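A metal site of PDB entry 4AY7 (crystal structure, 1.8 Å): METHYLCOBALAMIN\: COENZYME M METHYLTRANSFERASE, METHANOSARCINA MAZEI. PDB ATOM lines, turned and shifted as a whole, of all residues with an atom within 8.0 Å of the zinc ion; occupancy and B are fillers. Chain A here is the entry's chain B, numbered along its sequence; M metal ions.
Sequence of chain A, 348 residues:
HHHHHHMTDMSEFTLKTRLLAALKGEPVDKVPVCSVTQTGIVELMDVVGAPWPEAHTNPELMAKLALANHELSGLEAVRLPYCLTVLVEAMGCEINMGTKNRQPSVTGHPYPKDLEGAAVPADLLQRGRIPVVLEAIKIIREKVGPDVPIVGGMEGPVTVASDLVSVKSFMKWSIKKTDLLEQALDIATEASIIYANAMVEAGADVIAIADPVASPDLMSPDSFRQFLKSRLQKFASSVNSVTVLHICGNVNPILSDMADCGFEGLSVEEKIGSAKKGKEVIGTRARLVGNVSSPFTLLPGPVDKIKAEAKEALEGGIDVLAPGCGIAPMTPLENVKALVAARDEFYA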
ATOM      1  N   THR A  37      -6.324  28.667 -24.832  1.00  0.00           N
ATOM      2  CA  THR A  37      -4.980  28.677 -24.284  1.00  0.00           C
ATOM      3  C   THR A  37      -4.389  30.068 -24.520  1.00  0.00           C
ATOM      4  O   THR A  37      -5.026  30.933 -25.135  1.00  0.00           O
ATOM      5  CB  THR A  37      -4.123  27.578 -24.971  1.00  0.00           C
ATOM      6  OG1 THR A  37      -4.158  27.779 -26.387  1.00  0.00           O
ATOM      7  CG2 THR A  37      -4.638  26.157 -24.647  1.00  0.00           C
ATOM      8  N   LEU A  84       0.675  30.416 -16.170  1.00  0.00           N
ATOM      9  CA  LEU A  84       0.078  29.417 -15.327  1.00  0.00           C
ATOM     10  C   LEU A  84       0.584  29.614 -13.858  1.00  0.00           C
ATOM     11  O   LEU A  84       0.864  28.619 -13.148  1.00  0.00           O
ATOM     12  CB  LEU A  84       0.474  28.041 -15.856  1.00  0.00           C
ATOM     13  CG  LEU A  84      -0.165  27.573 -17.153  1.00  0.00           C
ATOM     14  CD1 LEU A  84       0.109  26.071 -17.334  1.00  0.00           C
ATOM     15  CD2 LEU A  84      -1.664  27.925 -17.098  1.00  0.00           C
ATOM     16  N   ALA A 210      -5.394  24.608 -17.580  1.00  0.00           N
ATOM     17  CA  ALA A 210      -4.319  23.872 -18.191  1.00  0.00           C
ATOM     18  C   ALA A 210      -3.692  23.168 -17.057  1.00  0.00           C
ATOM     19  O   ALA A 210      -3.269  23.848 -16.055  1.00  0.00           O
ATOM     20  CB  ALA A 210      -3.291  24.815 -18.840  1.00  0.00           C
ATOM     21  N   ASP A 211      -3.589  21.843 -17.195  1.00  0.00           N
ATOM     22  CA  ASP A 211      -3.014  21.051 -16.141  1.00  0.00           C
ATOM     23  C   ASP A 211      -1.906  20.099 -16.651  1.00  0.00           C
ATOM     24  O   ASP A 211      -2.065  18.885 -16.637  1.00  0.00           O
ATOM     25  CB  ASP A 211      -4.145  20.329 -15.443  1.00  0.00           C
ATOM     26  CG  ASP A 211      -3.962  20.264 -13.926  1.00  0.00           C
ATOM     27  OD1 ASP A 211      -2.869  20.495 -13.479  1.00  0.00           O
ATOM     28  OD2 ASP A 211      -4.892  19.927 -13.183  1.00  0.00           O
ATOM     29  N   PRO A 212      -0.727  20.667 -16.961  1.00  0.00           N
ATOM     30  CA  PRO A 212       0.397  19.913 -17.550  1.00  0.00           C
ATOM     31  C   PRO A 212       0.931  18.745 -16.708  1.00  0.00           C
ATOM     32  O   PRO A 212       1.441  17.776 -17.240  1.00  0.00           O
ATOM     33  CB  PRO A 212       1.442  20.982 -17.805  1.00  0.00           C
ATOM     34  CG  PRO A 212       1.042  22.114 -16.917  1.00  0.00           C
ATOM     35  CD  PRO A 212      -0.441  22.112 -16.935  1.00  0.00           C
ATOM     36  N   HIS A 246      -7.499  21.353 -20.479  1.00  0.00           N
ATOM     37  CA  HIS A 246      -6.408  21.207 -21.445  1.00  0.00           C
ATOM     38  C   HIS A 246      -5.311  20.516 -20.737  1.00  0.00           C
ATOM     39  O   HIS A 246      -4.772  21.027 -19.734  1.00  0.00           O
ATOM     40  CB  HIS A 246      -5.984  22.537 -21.955  1.00  0.00           C
ATOM     41  CG  HIS A 246      -4.737  22.455 -22.826  1.00  0.00           C
ATOM     42  ND1 HIS A 246      -4.770  22.240 -24.146  1.00  0.00           N
ATOM     43  CD2 HIS A 246      -3.390  22.513 -22.475  1.00  0.00           C
ATOM     44  CE1 HIS A 246      -3.485  22.136 -24.610  1.00  0.00           C
ATOM     45  NE2 HIS A 246      -2.671  22.355 -23.604  1.00  0.00           N
ATOM     46  N   ILE A 247      -4.996  19.308 -21.204  1.00  0.00           N
ATOM     47  CA  ILE A 247      -3.848  18.624 -20.686  1.00  0.00           C
ATOM     48  C   ILE A 247      -2.883  18.449 -21.825  1.00  0.00           C
ATOM     49  O   ILE A 247      -3.270  18.039 -22.915  1.00  0.00           O
ATOM     50  CB  ILE A 247      -4.194  17.280 -20.000  1.00  0.00           C
ATOM     51  CG1 ILE A 247      -5.066  17.551 -18.784  1.00  0.00           C
ATOM     52  CG2 ILE A 247      -2.901  16.538 -19.599  1.00  0.00           C
ATOM     53  CD1 ILE A 247      -5.533  16.308 -18.058  1.00  0.00           C
ATOM     54  N   CYS A 248      -1.632  18.850 -21.594  1.00  0.00           N
ATOM     55  CA  CYS A 248      -0.575  18.784 -22.610  1.00  0.00           C
ATOM     56  C   CYS A 248      -0.111  17.350 -22.934  1.00  0.00           C
ATOM     57  O   CYS A 248      -0.138  16.429 -22.078  1.00  0.00           O
ATOM     58  CB  CYS A 248       0.689  19.538 -22.080  1.00  0.00           C
ATOM     59  SG  CYS A 248       0.393  21.246 -21.519  1.00  0.00           S
ATOM     60  N   GLY A 249       0.410  17.205 -24.127  1.00  0.00           N
ATOM     61  CA  GLY A 249       1.100  15.990 -24.541  1.00  0.00           C
ATOM     62  C   GLY A 249       0.179  15.000 -25.246  1.00  0.00           C
ATOM     63  O   GLY A 249      -0.910  15.356 -25.801  1.00  0.00           O
ATOM     64  N   SER A 267      -9.466  20.376 -24.453  1.00  0.00           N
ATOM     65  CA  SER A 267      -8.528  21.032 -25.390  1.00  0.00           C
ATOM     66  C   SER A 267      -7.321  20.103 -25.514  1.00  0.00           C
ATOM     67  O   SER A 267      -6.661  19.718 -24.499  1.00  0.00           O
ATOM     68  CB  SER A 267      -8.154  22.426 -24.892  1.00  0.00           C
ATOM     69  OG  SER A 267      -6.935  22.837 -25.465  1.00  0.00           O
ATOM     70  N   VAL A 268      -7.066  19.671 -26.727  1.00  0.00           N
ATOM     71  CA  VAL A 268      -6.039  18.673 -26.998  1.00  0.00           C
ATOM     72  C   VAL A 268      -5.099  19.228 -28.088  1.00  0.00           C
ATOM     73  O   VAL A 268      -5.507  20.063 -28.943  1.00  0.00           O
ATOM     74  CB  VAL A 268      -6.674  17.359 -27.515  1.00  0.00           C
ATOM     75  CG1 VAL A 268      -7.746  16.871 -26.575  1.00  0.00           C
ATOM     76  CG2 VAL A 268      -7.372  17.617 -28.843  1.00  0.00           C
ATOM     77  N   GLU A 269      -3.846  18.739 -28.019  1.00  0.00           N
ATOM     78  CA  GLU A 269      -2.794  19.018 -28.990  1.00  0.00           C
ATOM     79  C   GLU A 269      -2.919  18.088 -30.207  1.00  0.00           C
ATOM     80  O   GLU A 269      -3.617  17.050 -30.153  1.00  0.00           O
ATOM     81  CB  GLU A 269      -1.394  18.902 -28.312  1.00  0.00           C
ATOM     82  CG  GLU A 269      -1.140  19.830 -27.130  1.00  0.00           C
ATOM     83  CD  GLU A 269       0.191  19.547 -26.400  1.00  0.00           C
ATOM     84  OE1 GLU A 269       1.057  18.866 -27.024  1.00  0.00           O
ATOM     85  OE2 GLU A 269       0.357  20.021 -25.209  1.00  0.00           O
ATOM     86  N   GLU A 270      -2.193  18.469 -31.273  1.00  0.00           N
ATOM     87  CA  GLU A 270      -2.058  17.698 -32.506  1.00  0.00           C
ATOM     88  C   GLU A 270      -1.527  16.276 -32.311  1.00  0.00           C
ATOM     89  O   GLU A 270      -1.861  15.360 -33.038  1.00  0.00           O
ATOM     90  CB  GLU A 270      -1.128  18.445 -33.501  1.00  0.00           C
ATOM     91  CG  GLU A 270       0.396  18.182 -33.373  1.00  0.00           C
ATOM     92  CD  GLU A 270       1.152  19.002 -32.252  1.00  0.00           C
ATOM     93  OE1 GLU A 270       0.611  19.206 -31.131  1.00  0.00           O
ATOM     94  OE2 GLU A 270       2.336  19.409 -32.502  1.00  0.00           O
ATOM     95  N   LYS A 271      -0.700  16.113 -31.298  1.00  0.00           N
ATOM     96  CA  LYS A 271      -0.019  14.857 -31.008  1.00  0.00           C
ATOM     97  C   LYS A 271      -0.948  13.672 -30.755  1.00  0.00           C
ATOM     98  O   LYS A 271      -0.563  12.577 -31.042  1.00  0.00           O
ATOM     99  CB  LYS A 271       0.926  15.015 -29.785  1.00  0.00           C
ATOM    100  CG  LYS A 271       2.144  15.864 -30.072  1.00  0.00           C
ATOM    101  CD  LYS A 271       2.892  16.313 -28.806  1.00  0.00           C
ATOM    102  CE  LYS A 271       3.286  17.809 -28.828  1.00  0.00           C
ATOM    103  NZ  LYS A 271       4.471  18.169 -29.689  1.00  0.00           N
ATOM    104  N   SER A 294       0.624  24.340 -32.129  1.00  0.00           N
ATOM    105  CA  SER A 294       1.246  25.639 -31.829  1.00  0.00           C
ATOM    106  C   SER A 294       2.685  25.718 -32.286  1.00  0.00           C
ATOM    107  O   SER A 294       3.019  26.595 -33.067  1.00  0.00           O
ATOM    108  CB  SER A 294       1.082  26.014 -30.387  1.00  0.00           C
ATOM    109  OG  SER A 294      -0.300  26.290 -30.193  1.00  0.00           O
ATOM    110  N   GLY A 324      -3.714  24.084 -30.577  1.00  0.00           N
ATOM    111  CA  GLY A 324      -3.581  22.875 -29.790  1.00  0.00           C
ATOM    112  C   GLY A 324      -2.983  23.098 -28.418  1.00  0.00           C
ATOM    113  O   GLY A 324      -3.282  22.319 -27.508  1.00  0.00           O
ATOM    114  N   CYS A 325      -2.153  24.105 -28.260  1.00  0.00           N
ATOM    115  CA  CYS A 325      -1.554  24.470 -26.958  1.00  0.00           C
ATOM    116  C   CYS A 325      -1.478  25.983 -26.900  1.00  0.00           C
ATOM    117  O   CYS A 325      -2.054  26.668 -27.734  1.00  0.00           O
ATOM    118  CB  CYS A 325      -0.162  23.840 -26.745  1.00  0.00           C
ATOM    119  SG  CYS A 325       0.367  23.823 -24.989  1.00  0.00           S
ATOM    120  N   GLY A 326      -0.780  26.538 -25.914  1.00  0.00           N
ATOM    121  CA  GLY A 326      -0.667  28.013 -25.891  1.00  0.00           C
ATOM    122  C   GLY A 326      -0.063  28.495 -27.197  1.00  0.00           C
ATOM    123  O   GLY A 326       0.759  27.825 -27.757  1.00  0.00           O
HETATM  124 ZN    ZN M   1      -0.471  21.961 -23.873  1.00  0.00          ZN
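O of Cys 325 is in hydrogen-bond range of OG1 of Thr 37, at 2.7 Å.
ND1 of His 246 lies within hydrogen-bond range of OG of Ser 267 (2.6 Å).
O of Cys 325 lies within hydrogen-bond range of OG of Ser 294 (3.0 Å).
N of Asp 211 lies within hydrogen-bond range of O of His 246, at 2.9 Å.
N of Gly 249 sits close to OE1 of Glu 269, at 3.4 Å.
Within 4 Å of the zinc ion: His 246, Cys 248, Glu 269 and Cys 325.
NE2 of His 246 binds the zinc ion (2.3 Å).
SG of Cys 325 binds the zinc ion, at 2.3 Å.
The side-chain carboxylate (OE2) of Glu 269 binds the zinc ion (2.5 Å).
The side-chain sulfur (SG) of Cys 248 is bound to the zinc ion (2.6 Å).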
